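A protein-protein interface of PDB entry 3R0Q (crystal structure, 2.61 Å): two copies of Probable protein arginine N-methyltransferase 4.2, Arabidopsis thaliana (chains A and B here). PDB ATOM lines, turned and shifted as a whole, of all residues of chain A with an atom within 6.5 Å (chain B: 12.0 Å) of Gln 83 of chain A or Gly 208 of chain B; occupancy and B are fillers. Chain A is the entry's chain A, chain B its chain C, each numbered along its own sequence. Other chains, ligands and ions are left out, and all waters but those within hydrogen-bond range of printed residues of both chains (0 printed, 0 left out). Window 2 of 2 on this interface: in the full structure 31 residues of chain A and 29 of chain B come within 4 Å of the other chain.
The indole nitrogen (NE1) of Trp 80 of chain A is in hydrogen-bond range of the backbone carbonyl oxygen (O) of Tyr 207 of chain B (3.4 Å).
N of Asp 210 of chain B is in hydrogen-bond range of OD1 of Asn 108 of chain A (2.8 Å).
O of Ile 203 of chain B is in hydrogen-bond range of N of Gly 208 of chain B (3.4 Å).
O of Ile 203 of chain B sits at hydrogen-bond distance from N of Val 209 of chain B (3.3 Å).
The backbone NH (N) of Gly 212 of chain B sits at hydrogen-bond distance from the side-chain carboxylate (OD1) of Asp 210 of chain B (3.3 Å).
Phe 52 of chain A touches Tyr 207 of chain B (CE1 to CA, 3.8 Å).
Val 209 of chain B touches Ile 79 of chain A (CG1 to CD1, 3.7 Å).
NE1 of Trp 80 of chain A touches CG2 of Val 209 of chain B, at 3.7 Å.
OE1 of Gln 83 of chain A touches O of Tyr 207 of chain B, 3.5 Å away.
Gln 83 of chain A touches Gly 208 of chain B.
OD1 of Asn 108 of chain A touches CA of Val 209 of chain B (3.5 Å).
Of chain B, only Val 209 (3.7 Å) comes within 4 Å of Ile 79 of chain A.
Ala 84 of chain A touches none of the printed residues of chain B.
No residue of chain B comes within 4 Å of Gly 85 of chain A.
No residue of chain B comes within 4 Å of Ala 86 of chain A.
Printed residues of chain B within 4 Å of Trp 80 of chain A: Tyr 207 and Val 209.
Printed residues of chain B within 4 Å of Phe 52 of chain A: Tyr 207 (3.8 Å).
Of the printed residues of chain A, Val 209 of chain B touches Ile 79 (3.7 Å), Trp 80 (3.7 Å) and Asn 108 (3.5 Å).
Printed residues of chain A within 4 Å of Tyr 207 of chain B: Phe 52, Trp 80 and Gln 83.
The nearest residue of chain B that does not touch Gln 83 of chain A is Val 209 of chain B (4.7 Å).
The nearest residue of chain A that does not touch Gly 208 of chain B is Asn 108 of chain A (4.2 Å).
Of the 15 printed residues of chain A, 5 touch a printed residue of chain B.
Hydrophobic or aromatic side chains of chain A that line the printed part of chain B: Phe 52, Ile 79 and Trp 80.
Of the 16 printed residues of chain B, 4 touch a printed residue of chain A.
Along chain B the printed residues that touch a printed residue of chain A span positions 207 to 210.
Among the printed residues, 8 pairs touch across the chains.
Among the printed residues, no Asp or Glu carboxylate lies within 4 Å of a Lys or Arg side-chain nitrogen of the other chain.
No position is printed for both chains.
Of the 8 pairs that touch across the chains among the printed residues, none has its exchanged pair printed and touching as well.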
ATOM      1  N   PHE A  52      31.037   8.898 -25.867  1.00  0.00           N
ATOM      2  CA  PHE A  52      29.666   8.786 -25.404  1.00  0.00           C
ATOM      3  C   PHE A  52      29.585   7.953 -24.121  1.00  0.00           C
ATOM      4  O   PHE A  52      28.982   8.376 -23.121  1.00  0.00           O
ATOM      5  CB  PHE A  52      28.827   8.169 -26.521  1.00  0.00           C
ATOM      6  CG  PHE A  52      27.433   7.801 -26.118  1.00  0.00           C
ATOM      7  CD1 PHE A  52      26.493   8.780 -25.878  1.00  0.00           C
ATOM      8  CD2 PHE A  52      27.054   6.475 -26.022  1.00  0.00           C
ATOM      9  CE1 PHE A  52      25.208   8.445 -25.526  1.00  0.00           C
ATOM     10  CE2 PHE A  52      25.773   6.136 -25.669  1.00  0.00           C
ATOM     11  CZ  PHE A  52      24.848   7.123 -25.424  1.00  0.00           C
ATOM     12  N   PHE A  56      28.544   9.007 -20.058  1.00  0.00           N
ATOM     13  CA  PHE A  56      27.356   8.431 -19.436  1.00  0.00           C
ATOM     14  C   PHE A  56      27.647   7.347 -18.392  1.00  0.00           C
ATOM     15  O   PHE A  56      26.847   7.137 -17.476  1.00  0.00           O
ATOM     16  CB  PHE A  56      26.381   7.945 -20.514  1.00  0.00           C
ATOM     17  CG  PHE A  56      25.711   9.072 -21.265  1.00  0.00           C
ATOM     18  CD1 PHE A  56      24.699   9.788 -20.678  1.00  0.00           C
ATOM     19  CD2 PHE A  56      26.111   9.422 -22.546  1.00  0.00           C
ATOM     20  CE1 PHE A  56      24.087  10.836 -21.345  1.00  0.00           C
ATOM     21  CE2 PHE A  56      25.499  10.470 -23.213  1.00  0.00           C
ATOM     22  CZ  PHE A  56      24.484  11.179 -22.606  1.00  0.00           C
ATOM     23  N   ALA A  78      29.572  18.771 -25.851  1.00  0.00           N
ATOM     24  CA  ALA A  78      28.846  19.722 -25.016  1.00  0.00           C
ATOM     25  C   ALA A  78      27.430  19.221 -24.773  1.00  0.00           C
ATOM     26  O   ALA A  78      26.912  19.252 -23.659  1.00  0.00           O
ATOM     27  CB  ALA A  78      28.800  21.082 -25.693  1.00  0.00           C
ATOM     28  N   ILE A  79      26.809  18.746 -25.839  1.00  0.00           N
ATOM     29  CA  ILE A  79      25.440  18.268 -25.769  1.00  0.00           C
ATOM     30  C   ILE A  79      25.298  17.106 -24.794  1.00  0.00           C
ATOM     31  O   ILE A  79      24.437  17.127 -23.925  1.00  0.00           O
ATOM     32  CB  ILE A  79      24.947  17.856 -27.150  1.00  0.00           C
ATOM     33  CG1 ILE A  79      24.785  19.107 -28.019  1.00  0.00           C
ATOM     34  CG2 ILE A  79      23.655  17.070 -27.026  1.00  0.00           C
ATOM     35  CD1 ILE A  79      24.366  18.832 -29.443  1.00  0.00           C
ATOM     36  N   TRP A  80      26.159  16.105 -24.935  1.00  0.00           N
ATOM     37  CA  TRP A  80      26.144  14.942 -24.057  1.00  0.00           C
ATOM     38  C   TRP A  80      26.376  15.335 -22.605  1.00  0.00           C
ATOM     39  O   TRP A  80      25.610  14.966 -21.716  1.00  0.00           O
ATOM     40  CB  TRP A  80      27.211  13.954 -24.507  1.00  0.00           C
ATOM     41  CG  TRP A  80      26.854  13.234 -25.762  1.00  0.00           C
ATOM     42  CD1 TRP A  80      25.601  13.044 -26.263  1.00  0.00           C
ATOM     43  CD2 TRP A  80      27.753  12.603 -26.677  1.00  0.00           C
ATOM     44  NE1 TRP A  80      25.660  12.326 -27.433  1.00  0.00           N
ATOM     45  CE2 TRP A  80      26.970  12.038 -27.709  1.00  0.00           C
ATOM     46  CE3 TRP A  80      29.143  12.447 -26.721  1.00  0.00           C
ATOM     47  CZ2 TRP A  80      27.529  11.338 -28.778  1.00  0.00           C
ATOM     48  CZ3 TRP A  80      29.697  11.745 -27.790  1.00  0.00           C
ATOM     49  CH2 TRP A  80      28.887  11.201 -28.799  1.00  0.00           C
ATOM     50  N   SER A  81      27.433  16.097 -22.363  1.00  0.00           N
ATOM     51  CA  SER A  81      27.696  16.599 -21.021  1.00  0.00           C
ATOM     52  C   SER A  81      26.431  17.179 -20.405  1.00  0.00           C
ATOM     53  O   SER A  81      26.059  16.833 -19.286  1.00  0.00           O
ATOM     54  CB  SER A  81      28.794  17.647 -21.065  1.00  0.00           C
ATOM     55  OG  SER A  81      29.960  17.094 -21.650  1.00  0.00           O
ATOM     56  N   ALA A  82      25.769  18.057 -21.150  1.00  0.00           N
ATOM     57  CA  ALA A  82      24.549  18.693 -20.673  1.00  0.00           C
ATOM     58  C   ALA A  82      23.461  17.644 -20.472  1.00  0.00           C
ATOM     59  O   ALA A  82      22.697  17.699 -19.513  1.00  0.00           O
ATOM     60  CB  ALA A  82      24.090  19.776 -21.649  1.00  0.00           C
ATOM     61  N   GLN A  83      23.401  16.676 -21.376  1.00  0.00           N
ATOM     62  CA  GLN A  83      22.465  15.567 -21.217  1.00  0.00           C
ATOM     63  C   GLN A  83      22.744  14.771 -19.939  1.00  0.00           C
ATOM     64  O   GLN A  83      21.831  14.198 -19.342  1.00  0.00           O
ATOM     65  CB  GLN A  83      22.518  14.655 -22.430  1.00  0.00           C
ATOM     66  CG  GLN A  83      22.158  15.367 -23.708  1.00  0.00           C
ATOM     67  CD  GLN A  83      21.807  14.414 -24.813  1.00  0.00           C
ATOM     68  OE1 GLN A  83      22.403  13.342 -24.940  1.00  0.00           O
ATOM     69  NE2 GLN A  83      20.818  14.783 -25.613  1.00  0.00           N
ATOM     70  N   ALA A  84      24.011  14.749 -19.521  1.00  0.00           N
ATOM     71  CA  ALA A  84      24.435  14.028 -18.317  1.00  0.00           C
ATOM     72  C   ALA A  84      24.280  14.838 -17.023  1.00  0.00           C
ATOM     73  O   ALA A  84      24.798  14.450 -15.968  1.00  0.00           O
ATOM     74  CB  ALA A  84      25.864  13.560 -18.466  1.00  0.00           C
ATOM     75  N   GLY A  85      23.588  15.971 -17.111  1.00  0.00           N
ATOM     76  CA  GLY A  85      23.185  16.706 -15.922  1.00  0.00           C
ATOM     77  C   GLY A  85      24.115  17.812 -15.470  1.00  0.00           C
ATOM     78  O   GLY A  85      23.989  18.312 -14.349  1.00  0.00           O
ATOM     79  N   ALA A  86      25.045  18.210 -16.328  1.00  0.00           N
ATOM     80  CA  ALA A  86      25.944  19.304 -15.987  1.00  0.00           C
ATOM     81  C   ALA A  86      25.146  20.526 -15.553  1.00  0.00           C
ATOM     82  O   ALA A  86      23.959  20.657 -15.880  1.00  0.00           O
ATOM     83  CB  ALA A  86      26.837  19.642 -17.149  1.00  0.00           C
ATOM     84  N   VAL A  89      27.671  24.075 -19.347  1.00  0.00           N
ATOM     85  CA  VAL A  89      28.714  23.595 -20.249  1.00  0.00           C
ATOM     86  C   VAL A  89      29.323  24.773 -21.032  1.00  0.00           C
ATOM     87  O   VAL A  89      28.619  25.719 -21.392  1.00  0.00           O
ATOM     88  CB  VAL A  89      28.134  22.535 -21.239  1.00  0.00           C
ATOM     89  CG1 VAL A  89      29.215  21.993 -22.163  1.00  0.00           C
ATOM     90  CG2 VAL A  89      27.468  21.397 -20.471  1.00  0.00           C
ATOM     91  N   ASN A 108      17.933  21.140 -29.676  1.00  0.00           N
ATOM     92  CA  ASN A 108      17.810  19.996 -28.787  1.00  0.00           C
ATOM     93  C   ASN A 108      17.502  20.451 -27.348  1.00  0.00           C
ATOM     94  O   ASN A 108      17.821  19.765 -26.371  1.00  0.00           O
ATOM     95  CB  ASN A 108      19.068  19.118 -28.862  1.00  0.00           C
ATOM     96  CG  ASN A 108      19.148  18.339 -30.174  1.00  0.00           C
ATOM     97  OD1 ASN A 108      19.158  17.022 -30.090  1.00  0.00           O
ATOM     98  ND2 ASN A 108      19.214  18.939 -31.261  1.00  0.00           N
ATOM     99  N   LEU A 110      18.731  22.598 -25.214  1.00  0.00           N
ATOM    100  CA  LEU A 110      19.828  22.639 -24.242  1.00  0.00           C
ATOM    101  C   LEU A 110      20.542  23.983 -24.183  1.00  0.00           C
ATOM    102  O   LEU A 110      21.628  24.074 -23.618  1.00  0.00           O
ATOM    103  CB  LEU A 110      20.866  21.556 -24.548  1.00  0.00           C
ATOM    104  CG  LEU A 110      20.411  20.103 -24.492  1.00  0.00           C
ATOM    105  CD1 LEU A 110      21.434  19.259 -25.227  1.00  0.00           C
ATOM    106  CD2 LEU A 110      20.249  19.654 -23.052  1.00  0.00           C
ATOM    107  N   ILE A 113      21.872  25.477 -20.825  1.00  0.00           N
ATOM    108  CA  ILE A 113      22.987  24.845 -20.142  1.00  0.00           C
ATOM    109  C   ILE A 113      24.277  25.013 -20.920  1.00  0.00           C
ATOM    110  O   ILE A 113      25.350  25.213 -20.340  1.00  0.00           O
ATOM    111  CB  ILE A 113      22.716  23.361 -19.900  1.00  0.00           C
ATOM    112  CG1 ILE A 113      21.592  23.212 -18.873  1.00  0.00           C
ATOM    113  CG2 ILE A 113      23.972  22.669 -19.414  1.00  0.00           C
ATOM    114  CD1 ILE A 113      21.649  21.937 -18.105  1.00  0.00           C
ATOM    115  N   ASN B 198      20.489   9.424 -43.629  1.00  0.00           N
ATOM    116  CA  ASN B 198      20.733   8.180 -42.906  1.00  0.00           C
ATOM    117  C   ASN B 198      21.524   8.471 -41.641  1.00  0.00           C
ATOM    118  O   ASN B 198      21.172   8.070 -40.539  1.00  0.00           O
ATOM    119  CB  ASN B 198      21.510   7.207 -43.775  1.00  0.00           C
ATOM    120  CG  ASN B 198      20.663   6.628 -44.879  1.00  0.00           C
ATOM    121  OD1 ASN B 198      19.513   6.258 -44.654  1.00  0.00           O
ATOM    122  ND2 ASN B 198      21.216   6.558 -46.083  1.00  0.00           N
ATOM    123  N   PHE B 199      22.609   9.192 -41.836  1.00  0.00           N
ATOM    124  CA  PHE B 199      23.500   9.610 -40.776  1.00  0.00           C
ATOM    125  C   PHE B 199      22.782  10.336 -39.640  1.00  0.00           C
ATOM    126  O   PHE B 199      23.030  10.059 -38.467  1.00  0.00           O
ATOM    127  CB  PHE B 199      24.581  10.480 -41.412  1.00  0.00           C
ATOM    128  CG  PHE B 199      25.302  11.369 -40.462  1.00  0.00           C
ATOM    129  CD1 PHE B 199      26.410  10.911 -39.778  1.00  0.00           C
ATOM    130  CD2 PHE B 199      24.915  12.691 -40.300  1.00  0.00           C
ATOM    131  CE1 PHE B 199      27.100  11.746 -38.914  1.00  0.00           C
ATOM    132  CE2 PHE B 199      25.594  13.531 -39.441  1.00  0.00           C
ATOM    133  CZ  PHE B 199      26.685  13.055 -38.743  1.00  0.00           C
ATOM    134  N   SER B 200      21.902  11.275 -39.959  1.00  0.00           N
ATOM    135  CA  SER B 200      21.181  11.972 -38.883  1.00  0.00           C
ATOM    136  C   SER B 200      20.153  11.059 -38.183  1.00  0.00           C
ATOM    137  O   SER B 200      19.833  11.252 -37.008  1.00  0.00           O
ATOM    138  CB  SER B 200      20.550  13.287 -39.372  1.00  0.00           C
ATOM    139  OG  SER B 200      20.046  13.179 -40.685  1.00  0.00           O
ATOM    140  N   ASP B 201      19.644  10.077 -38.920  1.00  0.00           N
ATOM    141  CA  ASP B 201      18.829   9.002 -38.348  1.00  0.00           C
ATOM    142  C   ASP B 201      19.670   8.142 -37.418  1.00  0.00           C
ATOM    143  O   ASP B 201      19.247   7.794 -36.318  1.00  0.00           O
ATOM    144  CB  ASP B 201      18.240   8.116 -39.447  1.00  0.00           C
ATOM    145  CG  ASP B 201      16.813   8.492 -39.800  1.00  0.00           C
ATOM    146  OD1 ASP B 201      16.434   9.674 -39.635  1.00  0.00           O
ATOM    147  OD2 ASP B 201      16.072   7.592 -40.250  1.00  0.00           O
ATOM    148  N   GLU B 202      20.870   7.798 -37.867  1.00  0.00           N
ATOM    149  CA  GLU B 202      21.769   7.009 -37.042  1.00  0.00           C
ATOM    150  C   GLU B 202      22.069   7.752 -35.740  1.00  0.00           C
ATOM    151  O   GLU B 202      21.894   7.205 -34.649  1.00  0.00           O
ATOM    152  CB  GLU B 202      23.052   6.664 -37.805  1.00  0.00           C
ATOM    153  N   ILE B 203      22.477   9.010 -35.858  1.00  0.00           N
ATOM    154  CA  ILE B 203      22.818   9.832 -34.691  1.00  0.00           C
ATOM    155  C   ILE B 203      21.619  10.168 -33.799  1.00  0.00           C
ATOM    156  O   ILE B 203      21.783  10.600 -32.657  1.00  0.00           O
ATOM    157  CB  ILE B 203      23.509  11.143 -35.118  1.00  0.00           C
ATOM    158  CG1 ILE B 203      24.887  10.841 -35.703  1.00  0.00           C
ATOM    159  CG2 ILE B 203      23.621  12.096 -33.952  1.00  0.00           C
ATOM    160  CD1 ILE B 203      25.828  12.031 -35.700  1.00  0.00           C
ATOM    161  N   LYS B 204      20.410   9.987 -34.311  1.00  0.00           N
ATOM    162  CA  LYS B 204      19.240  10.206 -33.469  1.00  0.00           C
ATOM    163  C   LYS B 204      18.899   8.936 -32.672  1.00  0.00           C
ATOM    164  O   LYS B 204      18.333   9.009 -31.583  1.00  0.00           O
ATOM    165  CB  LYS B 204      18.042  10.677 -34.298  1.00  0.00           C
ATOM    166  N   SER B 205      19.255   7.776 -33.223  1.00  0.00           N
ATOM    167  CA  SER B 205      18.955   6.491 -32.593  1.00  0.00           C
ATOM    168  C   SER B 205      19.919   6.189 -31.459  1.00  0.00           C
ATOM    169  O   SER B 205      19.505   5.785 -30.368  1.00  0.00           O
ATOM    170  CB  SER B 205      19.007   5.362 -33.621  1.00  0.00           C
ATOM    171  OG  SER B 205      17.912   5.450 -34.504  1.00  0.00           O
ATOM    172  N   TYR B 206      21.209   6.362 -31.743  1.00  0.00           N
ATOM    173  CA  TYR B 206      22.261   6.257 -30.746  1.00  0.00           C
ATOM    174  C   TYR B 206      22.664   7.680 -30.445  1.00  0.00           C
ATOM    175  O   TYR B 206      22.469   8.549 -31.286  1.00  0.00           O
ATOM    176  CB  TYR B 206      23.437   5.457 -31.305  1.00  0.00           C
ATOM    177  CG  TYR B 206      23.091   4.000 -31.530  1.00  0.00           C
ATOM    178  CD1 TYR B 206      22.216   3.337 -30.668  1.00  0.00           C
ATOM    179  CD2 TYR B 206      23.616   3.295 -32.608  1.00  0.00           C
ATOM    180  CE1 TYR B 206      21.879   2.009 -30.859  1.00  0.00           C
ATOM    181  CE2 TYR B 206      23.285   1.952 -32.812  1.00  0.00           C
ATOM    182  CZ  TYR B 206      22.414   1.317 -31.925  1.00  0.00           C
ATOM    183  OH  TYR B 206      22.061  -0.007 -32.096  1.00  0.00           O
ATOM    184  N   TYR B 207      23.186   7.936 -29.252  1.00  0.00           N
ATOM    185  CA  TYR B 207      23.616   9.290 -28.872  1.00  0.00           C
ATOM    186  C   TYR B 207      22.445  10.221 -28.550  1.00  0.00           C
ATOM    187  O   TYR B 207      22.516  11.032 -27.617  1.00  0.00           O
ATOM    188  CB  TYR B 207      24.504   9.889 -29.961  1.00  0.00           C
ATOM    189  CG  TYR B 207      25.423   8.862 -30.578  1.00  0.00           C
ATOM    190  CD1 TYR B 207      26.306   8.128 -29.789  1.00  0.00           C
ATOM    191  CD2 TYR B 207      25.397   8.603 -31.945  1.00  0.00           C
ATOM    192  CE1 TYR B 207      27.142   7.179 -30.345  1.00  0.00           C
ATOM    193  CE2 TYR B 207      26.234   7.650 -32.511  1.00  0.00           C
ATOM    194  CZ  TYR B 207      27.102   6.946 -31.699  1.00  0.00           C
ATOM    195  OH  TYR B 207      27.937   5.996 -32.223  1.00  0.00           O
ATOM    196  N   GLY B 208      21.364  10.099 -29.313  1.00  0.00           N
ATOM    197  CA  GLY B 208      20.135  10.808 -29.003  1.00  0.00           C
ATOM    198  C   GLY B 208      20.184  12.304 -29.263  1.00  0.00           C
ATOM    199  O   GLY B 208      19.481  13.078 -28.611  1.00  0.00           O
ATOM    200  N   VAL B 209      21.024  12.710 -30.210  1.00  0.00           N
ATOM    201  CA  VAL B 209      21.061  14.095 -30.663  1.00  0.00           C
ATOM    202  C   VAL B 209      20.345  14.182 -32.002  1.00  0.00           C
ATOM    203  O   VAL B 209      20.473  13.300 -32.840  1.00  0.00           O
ATOM    204  CB  VAL B 209      22.495  14.621 -30.813  1.00  0.00           C
ATOM    205  CG1 VAL B 209      22.487  16.127 -31.067  1.00  0.00           C
ATOM    206  CG2 VAL B 209      23.319  14.294 -29.566  1.00  0.00           C
ATOM    207  N   ASP B 210      19.577  15.244 -32.192  1.00  0.00           N
ATOM    208  CA  ASP B 210      18.779  15.406 -33.395  1.00  0.00           C
ATOM    209  C   ASP B 210      19.496  16.382 -34.317  1.00  0.00           C
ATOM    210  O   ASP B 210      19.682  17.543 -33.969  1.00  0.00           O
ATOM    211  CB  ASP B 210      17.404  15.953 -33.016  1.00  0.00           C
ATOM    212  CG  ASP B 210      16.429  15.931 -34.170  1.00  0.00           C
ATOM    213  OD1 ASP B 210      16.852  15.594 -35.304  1.00  0.00           O
ATOM    214  OD2 ASP B 210      15.242  16.260 -33.935  1.00  0.00           O
ATOM    215  N   MET B 211      19.895  15.917 -35.492  1.00  0.00           N
ATOM    216  CA  MET B 211      20.724  16.726 -36.376  1.00  0.00           C
ATOM    217  C   MET B 211      19.934  17.436 -37.476  1.00  0.00           C
ATOM    218  O   MET B 211      20.515  17.864 -38.471  1.00  0.00           O
ATOM    219  CB  MET B 211      21.790  15.843 -37.026  1.00  0.00           C
ATOM    220  CG  MET B 211      22.650  15.077 -36.033  1.00  0.00           C
ATOM    221  SD  MET B 211      24.052  16.061 -35.500  1.00  0.00           S
ATOM    222  CE  MET B 211      24.200  15.544 -33.798  1.00  0.00           C
ATOM    223  N   GLY B 212      18.626  17.576 -37.300  1.00  0.00           N
ATOM    224  CA  GLY B 212      17.793  18.088 -38.366  1.00  0.00           C
ATOM    225  C   GLY B 212      18.106  19.492 -38.846  1.00  0.00           C
ATOM    226  O   GLY B 212      17.990  19.771 -40.035  1.00  0.00           O
ATOM    227  N   VAL B 213      18.494  20.380 -37.932  1.00  0.00           N
ATOM    228  CA  VAL B 213      18.563  21.812 -38.248  1.00  0.00           C
ATOM    229  C   VAL B 213      19.829  22.174 -38.983  1.00  0.00           C
ATOM    230  O   VAL B 213      20.021  23.328 -39.359  1.00  0.00           O
ATOM    231  CB  VAL B 213      18.469  22.703 -36.995  1.00  0.00           C
ATOM    232  CG1 VAL B 213      17.092  22.583 -36.353  1.00  0.00           C
ATOM    233  CG2 VAL B 213      19.570  22.341 -36.014  1.00  0.00           C
